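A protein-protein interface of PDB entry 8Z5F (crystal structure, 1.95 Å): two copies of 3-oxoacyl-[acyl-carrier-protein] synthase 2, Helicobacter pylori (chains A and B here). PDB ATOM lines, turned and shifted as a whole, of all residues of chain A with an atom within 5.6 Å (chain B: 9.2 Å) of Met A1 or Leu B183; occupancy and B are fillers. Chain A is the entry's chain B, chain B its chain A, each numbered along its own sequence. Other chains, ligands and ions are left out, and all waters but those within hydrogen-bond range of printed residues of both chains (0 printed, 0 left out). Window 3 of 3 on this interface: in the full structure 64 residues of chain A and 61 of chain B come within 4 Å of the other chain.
Printed residues of chain B that touch a printed residue of chain A: Lys B179, Thr B180 and Leu B183. Hydrophobic or aromatic side chains of chain B within 4 Å of the printed part of chain A: Leu B183. Of the 7 printed residues of chain A, 4 touch a printed residue of chain B. Among the printed residues, 6 pairs touch across the chains.
O of Glu B176 is in hydrogen-bond range of OG1 of Thr B180, at 2.7 Å. O of Thr B180 is in hydrogen-bond range of N of Gly B185 (2.8 Å).
Leu A182 touches none of the printed residues of chain B. Of the printed residues of chain B, Leu A183 touches Lys B179 and Leu B183. Printed residues of chain B within 4 Å of Tyr A264: Leu B183. Pro B159 touches none of the printed residues of chain A. Leu B183 touches just these residues of chain A: Met A1, Lys A179, Leu A183 and Tyr A264. The nearest printed residue of chain B that does not touch Tyr A264 is Gly B185 (5.9 Å).
Met A1 touches Leu B183, but with the chains exchanged Leu A183 does not touch Met B1 (4.1 Å). Lys A179 touches Leu B183, and with the chains exchanged Leu A183 touches Lys B179. Leu B183 touches its own counterpart, Leu A183. Tyr A264 touches Leu B183, but with the chains exchanged Leu A183 does not touch Tyr B264 (4.03 Å). Positions printed for both chains: 1, 2, 179, 182, 183 and 264.
Among the printed residues, pairs that only touch across the chains: Met A1 with Leu B183 (3.8 Å), Lys A179 with Leu B183 (3.5 Å), Leu A183 with Lys B179 (3.7 Å), Leu A183 with Leu B183 (3.7 Å) and Tyr A264 with Leu B183 (3.9 Å).
The side-chain amino group (NZ) of Lys A179 is in hydrogen-bond range of the side-chain hydroxyl (OG1) of Thr B180 (3.3 Å).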
ATOM      1  N   MET A   1      -2.797   5.359 -16.697  1.00  0.00           N
ATOM      2  CA  MET A   1      -1.595   5.867 -15.988  1.00  0.00           C
ATOM      3  C   MET A   1      -1.703   5.520 -14.503  1.00  0.00           C
ATOM      4  O   MET A   1      -2.670   4.835 -14.133  1.00  0.00           O
ATOM      5  CB  MET A   1      -1.478   7.386 -16.126  1.00  0.00           C
ATOM      6  CG  MET A   1      -0.294   7.835 -16.957  1.00  0.00           C
ATOM      7  SD  MET A   1      -0.545   7.541 -18.722  1.00  0.00           S
ATOM      8  CE  MET A   1      -1.089   9.164 -19.251  1.00  0.00           C
ATOM      9  N   ARG A   2      -0.752   5.991 -13.692  1.00  0.00           N
ATOM     10  CA  ARG A   2      -0.813   5.758 -12.224  1.00  0.00           C
ATOM     11  C   ARG A   2      -2.058   6.471 -11.689  1.00  0.00           C
ATOM     12  O   ARG A   2      -2.402   7.537 -12.232  1.00  0.00           O
ATOM     13  CB  ARG A   2       0.458   6.271 -11.538  1.00  0.00           C
ATOM     14  CG  ARG A   2       1.736   5.565 -11.965  1.00  0.00           C
ATOM     15  CD  ARG A   2       2.960   6.262 -11.402  1.00  0.00           C
ATOM     16  NE  ARG A   2       2.960   6.318  -9.948  1.00  0.00           N
ATOM     17  CZ  ARG A   2       3.896   6.915  -9.219  1.00  0.00           C
ATOM     18  NH1 ARG A   2       4.607   7.901  -9.732  1.00  0.00           N
ATOM     19  NH2 ARG A   2       4.114   6.526  -7.974  1.00  0.00           N
ATOM     20  N   ARG A   3      -2.715   5.904 -10.680  1.00  0.00           N
ATOM     21  CA  ARG A   3      -3.956   6.531 -10.183  1.00  0.00           C
ATOM     22  C   ARG A   3      -3.549   7.463  -9.043  1.00  0.00           C
ATOM     23  O   ARG A   3      -2.594   7.109  -8.328  1.00  0.00           O
ATOM     24  CB  ARG A   3      -4.963   5.438  -9.824  1.00  0.00           C
ATOM     25  CG  ARG A   3      -6.002   5.154 -10.899  1.00  0.00           C
ATOM     26  CD  ARG A   3      -6.839   3.926 -10.600  1.00  0.00           C
ATOM     27  NE  ARG A   3      -7.857   4.144  -9.581  1.00  0.00           N
ATOM     28  CZ  ARG A   3      -8.275   3.213  -8.731  1.00  0.00           C
ATOM     29  NH1 ARG A   3      -7.665   2.044  -8.686  1.00  0.00           N
ATOM     30  NH2 ARG A   3      -9.300   3.450  -7.932  1.00  0.00           N
ATOM     31  N   LYS A 179       1.094  15.661 -13.123  1.00  0.00           N
ATOM     32  CA  LYS A 179       2.064  15.309 -14.198  1.00  0.00           C
ATOM     33  C   LYS A 179       3.276  14.629 -13.602  1.00  0.00           C
ATOM     34  O   LYS A 179       3.729  13.621 -14.140  1.00  0.00           O
ATOM     35  CB  LYS A 179       2.560  16.569 -14.907  1.00  0.00           C
ATOM     36  CG  LYS A 179       1.774  17.011 -16.132  1.00  0.00           C
ATOM     37  CD  LYS A 179       2.240  18.333 -16.680  1.00  0.00           C
ATOM     38  CE  LYS A 179       1.312  18.901 -17.728  1.00  0.00           C
ATOM     39  NZ  LYS A 179       1.285  20.380 -17.687  1.00  0.00           N
ATOM     40  N   LEU A 182       2.200  11.111 -12.376  1.00  0.00           N
ATOM     41  CA  LEU A 182       1.919  10.295 -13.553  1.00  0.00           C
ATOM     42  C   LEU A 182       3.202   9.819 -14.227  1.00  0.00           C
ATOM     43  O   LEU A 182       3.293   8.663 -14.659  1.00  0.00           O
ATOM     44  CB  LEU A 182       1.066  11.067 -14.561  1.00  0.00           C
ATOM     45  CG  LEU A 182      -0.389  11.360 -14.207  1.00  0.00           C
ATOM     46  CD1 LEU A 182      -1.066  12.024 -15.383  1.00  0.00           C
ATOM     47  CD2 LEU A 182      -1.151  10.096 -13.795  1.00  0.00           C
ATOM     48  N   LEU A 183       4.206  10.689 -14.337  1.00  0.00           N
ATOM     49  CA  LEU A 183       5.434  10.273 -15.002  1.00  0.00           C
ATOM     50  C   LEU A 183       6.415   9.603 -14.055  1.00  0.00           C
ATOM     51  O   LEU A 183       7.584   9.420 -14.419  1.00  0.00           O
ATOM     52  CB  LEU A 183       6.097  11.457 -15.702  1.00  0.00           C
ATOM     53  CG  LEU A 183       5.267  11.955 -16.894  1.00  0.00           C
ATOM     54  CD1 LEU A 183       5.691  13.375 -17.274  1.00  0.00           C
ATOM     55  CD2 LEU A 183       5.422  11.026 -18.057  1.00  0.00           C
ATOM     56  N   TYR A 264      -7.676  16.770 -16.316  1.00  0.00           N
ATOM     57  CA  TYR A 264      -7.212  18.148 -16.326  1.00  0.00           C
ATOM     58  C   TYR A 264      -7.159  18.651 -17.760  1.00  0.00           C
ATOM     59  O   TYR A 264      -7.122  17.873 -18.717  1.00  0.00           O
ATOM     60  CB  TYR A 264      -5.842  18.317 -15.628  1.00  0.00           C
ATOM     61  CG  TYR A 264      -4.647  17.695 -16.328  1.00  0.00           C
ATOM     62  CD1 TYR A 264      -4.043  18.310 -17.430  1.00  0.00           C
ATOM     63  CD2 TYR A 264      -4.084  16.513 -15.856  1.00  0.00           C
ATOM     64  CE1 TYR A 264      -2.922  17.752 -18.049  1.00  0.00           C
ATOM     65  CE2 TYR A 264      -2.970  15.943 -16.472  1.00  0.00           C
ATOM     66  CZ  TYR A 264      -2.393  16.567 -17.567  1.00  0.00           C
ATOM     67  OH  TYR A 264      -1.300  15.984 -18.186  1.00  0.00           O
ATOM     68  N   MET B   1       9.156   6.903 -24.382  1.00  0.00           N
ATOM     69  CA  MET B   1       7.730   7.025 -24.750  1.00  0.00           C
ATOM     70  C   MET B   1       7.652   7.886 -26.006  1.00  0.00           C
ATOM     71  O   MET B   1       8.142   7.425 -27.042  1.00  0.00           O
ATOM     72  CB  MET B   1       6.957   7.678 -23.612  1.00  0.00           C
ATOM     73  CG  MET B   1       7.823   8.447 -22.648  1.00  0.00           C
ATOM     74  SD  MET B   1       6.743   9.444 -21.608  1.00  0.00           S
ATOM     75  CE  MET B   1       5.156   9.015 -22.320  1.00  0.00           C
ATOM     76  N   ARG B   2       7.073   9.081 -25.937  1.00  0.00           N
ATOM     77  CA  ARG B   2       7.121   9.955 -27.139  1.00  0.00           C
ATOM     78  C   ARG B   2       8.519  10.574 -27.156  1.00  0.00           C
ATOM     79  O   ARG B   2       9.017  10.920 -26.084  1.00  0.00           O
ATOM     80  CB  ARG B   2       6.033  11.025 -27.146  1.00  0.00           C
ATOM     81  CG  ARG B   2       4.758  10.631 -27.870  1.00  0.00           C
ATOM     82  CD  ARG B   2       3.573  11.299 -27.205  1.00  0.00           C
ATOM     83  NE  ARG B   2       3.598  12.744 -27.316  1.00  0.00           N
ATOM     84  CZ  ARG B   2       3.030  13.416 -28.306  1.00  0.00           C
ATOM     85  NH1 ARG B   2       2.663  12.777 -29.399  1.00  0.00           N
ATOM     86  NH2 ARG B   2       2.827  14.717 -28.200  1.00  0.00           N
ATOM     87  N   ARG B 103      -2.070  22.721 -30.561  1.00  0.00           N
ATOM     88  CA  ARG B 103      -1.174  21.703 -30.032  1.00  0.00           C
ATOM     89  C   ARG B 103       0.237  22.225 -29.825  1.00  0.00           C
ATOM     90  O   ARG B 103       1.149  21.429 -29.593  1.00  0.00           O
ATOM     91  CB  ARG B 103      -1.166  20.486 -30.952  1.00  0.00           C
ATOM     92  CG  ARG B 103      -2.517  19.783 -30.986  1.00  0.00           C
ATOM     93  CD  ARG B 103      -2.736  18.964 -29.721  1.00  0.00           C
ATOM     94  NE  ARG B 103      -1.792  17.854 -29.658  1.00  0.00           N
ATOM     95  CZ  ARG B 103      -1.615  17.076 -28.598  1.00  0.00           C
ATOM     96  NH1 ARG B 103      -2.351  17.222 -27.501  1.00  0.00           N
ATOM     97  NH2 ARG B 103      -0.672  16.139 -28.631  1.00  0.00           N
ATOM     98  N   PRO B 159      -0.988  24.416 -23.979  1.00  0.00           N
ATOM     99  CA  PRO B 159      -0.705  24.723 -22.566  1.00  0.00           C
ATOM    100  C   PRO B 159       0.270  25.884 -22.416  1.00  0.00           C
ATOM    101  O   PRO B 159       1.271  25.986 -23.125  1.00  0.00           O
ATOM    102  CB  PRO B 159      -0.114  23.410 -22.038  1.00  0.00           C
ATOM    103  CG  PRO B 159      -0.819  22.369 -22.840  1.00  0.00           C
ATOM    104  CD  PRO B 159      -0.900  22.971 -24.240  1.00  0.00           C
ATOM    105  N   ILE B 175      11.798  21.324 -18.479  1.00  0.00           N
ATOM    106  CA  ILE B 175      11.282  20.040 -18.002  1.00  0.00           C
ATOM    107  C   ILE B 175       9.752  20.009 -18.033  1.00  0.00           C
ATOM    108  O   ILE B 175       9.138  19.004 -18.430  1.00  0.00           O
ATOM    109  CB  ILE B 175      11.837  19.746 -16.593  1.00  0.00           C
ATOM    110  CG1 ILE B 175      13.351  19.491 -16.685  1.00  0.00           C
ATOM    111  CG2 ILE B 175      11.059  18.596 -15.934  1.00  0.00           C
ATOM    112  CD1 ILE B 175      14.074  19.518 -15.315  1.00  0.00           C
ATOM    113  N   GLU B 176       9.111  21.109 -17.651  1.00  0.00           N
ATOM    114  CA  GLU B 176       7.653  21.147 -17.673  1.00  0.00           C
ATOM    115  C   GLU B 176       7.124  21.055 -19.098  1.00  0.00           C
ATOM    116  O   GLU B 176       6.077  20.433 -19.336  1.00  0.00           O
ATOM    117  CB  GLU B 176       7.158  22.420 -16.974  1.00  0.00           C
ATOM    118  CG  GLU B 176       5.680  22.621 -17.040  1.00  0.00           C
ATOM    119  CD  GLU B 176       5.139  23.508 -15.924  1.00  0.00           C
ATOM    120  OE1 GLU B 176       5.684  24.615 -15.693  1.00  0.00           O
ATOM    121  OE2 GLU B 176       4.146  23.089 -15.282  1.00  0.00           O
ATOM    122  N   ALA B 177       7.852  21.635 -20.058  1.00  0.00           N
ATOM    123  CA  ALA B 177       7.474  21.476 -21.457  1.00  0.00           C
ATOM    124  C   ALA B 177       7.668  20.034 -21.920  1.00  0.00           C
ATOM    125  O   ALA B 177       6.822  19.486 -22.636  1.00  0.00           O
ATOM    126  CB  ALA B 177       8.290  22.425 -22.325  1.00  0.00           C
ATOM    127  N   VAL B 178       8.780  19.407 -21.524  1.00  0.00           N
ATOM    128  CA  VAL B 178       9.001  17.997 -21.851  1.00  0.00           C
ATOM    129  C   VAL B 178       7.888  17.137 -21.257  1.00  0.00           C
ATOM    130  O   VAL B 178       7.316  16.277 -21.931  1.00  0.00           O
ATOM    131  CB  VAL B 178      10.393  17.544 -21.363  1.00  0.00           C
ATOM    132  CG1 VAL B 178      10.452  16.005 -21.211  1.00  0.00           C
ATOM    133  CG2 VAL B 178      11.506  18.042 -22.310  1.00  0.00           C
ATOM    134  N   LYS B 179       7.556  17.364 -19.985  1.00  0.00           N
ATOM    135  CA  LYS B 179       6.504  16.576 -19.353  1.00  0.00           C
ATOM    136  C   LYS B 179       5.181  16.738 -20.098  1.00  0.00           C
ATOM    137  O   LYS B 179       4.465  15.759 -20.335  1.00  0.00           O
ATOM    138  CB  LYS B 179       6.331  16.998 -17.889  1.00  0.00           C
ATOM    139  CG  LYS B 179       7.476  16.634 -16.929  1.00  0.00           C
ATOM    140  CD  LYS B 179       7.027  16.939 -15.507  1.00  0.00           C
ATOM    141  CE  LYS B 179       8.177  16.871 -14.523  1.00  0.00           C
ATOM    142  NZ  LYS B 179       7.891  17.618 -13.257  1.00  0.00           N
ATOM    143  N   THR B 180       4.834  17.981 -20.448  1.00  0.00           N
ATOM    144  CA  THR B 180       3.597  18.250 -21.171  1.00  0.00           C
ATOM    145  C   THR B 180       3.529  17.451 -22.475  1.00  0.00           C
ATOM    146  O   THR B 180       2.495  16.844 -22.793  1.00  0.00           O
ATOM    147  CB  THR B 180       3.489  19.759 -21.426  1.00  0.00           C
ATOM    148  OG1 THR B 180       3.487  20.444 -20.161  1.00  0.00           O
ATOM    149  CG2 THR B 180       2.208  20.102 -22.180  1.00  0.00           C
ATOM    150  N   ILE B 181       4.628  17.429 -23.232  1.00  0.00           N
ATOM    151  CA  ILE B 181       4.673  16.695 -24.499  1.00  0.00           C
ATOM    152  C   ILE B 181       4.671  15.186 -24.254  1.00  0.00           C
ATOM    153  O   ILE B 181       3.989  14.435 -24.961  1.00  0.00           O
ATOM    154  CB  ILE B 181       5.903  17.125 -25.325  1.00  0.00           C
ATOM    155  CG1 ILE B 181       5.785  18.583 -25.784  1.00  0.00           C
ATOM    156  CG2 ILE B 181       6.073  16.232 -26.535  1.00  0.00           C
ATOM    157  CD1 ILE B 181       7.070  19.155 -26.406  1.00  0.00           C
ATOM    158  N   LEU B 182       5.417  14.720 -23.248  1.00  0.00           N
ATOM    159  CA  LEU B 182       5.413  13.294 -22.915  1.00  0.00           C
ATOM    160  C   LEU B 182       4.008  12.790 -22.592  1.00  0.00           C
ATOM    161  O   LEU B 182       3.652  11.671 -22.972  1.00  0.00           O
ATOM    162  CB  LEU B 182       6.346  13.008 -21.738  1.00  0.00           C
ATOM    163  CG  LEU B 182       7.863  13.055 -21.992  1.00  0.00           C
ATOM    164  CD1 LEU B 182       8.662  12.822 -20.678  1.00  0.00           C
ATOM    165  CD2 LEU B 182       8.281  12.063 -23.090  1.00  0.00           C
ATOM    166  N   LEU B 183       3.195  13.586 -21.890  1.00  0.00           N
ATOM    167  CA  LEU B 183       1.847  13.147 -21.539  1.00  0.00           C
ATOM    168  C   LEU B 183       0.820  13.503 -22.608  1.00  0.00           C
ATOM    169  O   LEU B 183      -0.382  13.489 -22.320  1.00  0.00           O
ATOM    170  CB  LEU B 183       1.420  13.723 -20.183  1.00  0.00           C
ATOM    171  CG  LEU B 183       2.153  13.094 -18.990  1.00  0.00           C
ATOM    172  CD1 LEU B 183       2.068  14.003 -17.799  1.00  0.00           C
ATOM    173  CD2 LEU B 183       1.613  11.717 -18.641  1.00  0.00           C
ATOM    174  N   ASN B 184       1.268  13.837 -23.820  1.00  0.00           N
ATOM    175  CA  ASN B 184       0.408  14.081 -24.979  1.00  0.00           C
ATOM    176  C   ASN B 184      -0.458  15.322 -24.815  1.00  0.00           C
ATOM    177  O   ASN B 184      -1.522  15.433 -25.445  1.00  0.00           O
ATOM    178  CB  ASN B 184      -0.501  12.881 -25.280  1.00  0.00           C
ATOM    179  CG  ASN B 184      -0.808  12.741 -26.758  1.00  0.00           C
ATOM    180  OD1 ASN B 184      -0.332  13.525 -27.592  1.00  0.00           O
ATOM    181  ND2 ASN B 184      -1.679  11.792 -27.081  1.00  0.00           N
ATOM    182  N   GLY B 185      -0.028  16.266 -23.977  1.00  0.00           N
ATOM    183  CA  GLY B 185      -0.734  17.526 -23.841  1.00  0.00           C
ATOM    184  C   GLY B 185      -0.417  18.531 -24.911  1.00  0.00           C
ATOM    185  O   GLY B 185      -1.090  19.559 -24.998  1.00  0.00           O
ATOM    186  N   ALA B 186       0.612  18.261 -25.710  1.00  0.00           N
ATOM    187  CA  ALA B 186       1.030  19.125 -26.799  1.00  0.00           C
ATOM    188  C   ALA B 186       1.947  18.324 -27.712  1.00  0.00           C
ATOM    189  O   ALA B 186       2.590  17.369 -27.276  1.00  0.00           O
ATOM    190  CB  ALA B 186       1.742  20.374 -26.274  1.00  0.00           C
ATOM    191  N   ASP B 187       2.011  18.724 -28.981  1.00  0.00           N
ATOM    192  CA  ASP B 187       2.997  18.166 -29.893  1.00  0.00           C
ATOM    193  C   ASP B 187       4.244  19.029 -30.012  1.00  0.00           C
ATOM    194  O   ASP B 187       5.294  18.522 -30.426  1.00  0.00           O
ATOM    195  CB  ASP B 187       2.379  17.962 -31.281  1.00  0.00           C
ATOM    196  CG  ASP B 187       1.166  17.042 -31.245  1.00  0.00           C
ATOM    197  OD1 ASP B 187       1.215  16.038 -30.505  1.00  0.00           O
ATOM    198  OD2 ASP B 187       0.169  17.320 -31.952  1.00  0.00           O
ATOM    199  N   TYR B 264      15.965  14.037 -17.547  1.00  0.00           N
ATOM    200  CA  TYR B 264      15.919  15.156 -16.616  1.00  0.00           C
ATOM    201  C   TYR B 264      15.861  14.615 -15.197  1.00  0.00           C
ATOM    202  O   TYR B 264      15.531  13.449 -14.971  1.00  0.00           O
ATOM    203  CB  TYR B 264      14.717  16.095 -16.867  1.00  0.00           C
ATOM    204  CG  TYR B 264      13.337  15.491 -16.648  1.00  0.00           C
ATOM    205  CD1 TYR B 264      12.777  15.384 -15.372  1.00  0.00           C
ATOM    206  CD2 TYR B 264      12.582  15.038 -17.729  1.00  0.00           C
ATOM    207  CE1 TYR B 264      11.502  14.825 -15.180  1.00  0.00           C
ATOM    208  CE2 TYR B 264      11.314  14.472 -17.550  1.00  0.00           C
ATOM    209  CZ  TYR B 264      10.785  14.366 -16.277  1.00  0.00           C
ATOM    210  OH  TYR B 264       9.529  13.817 -16.125  1.00  0.00           O
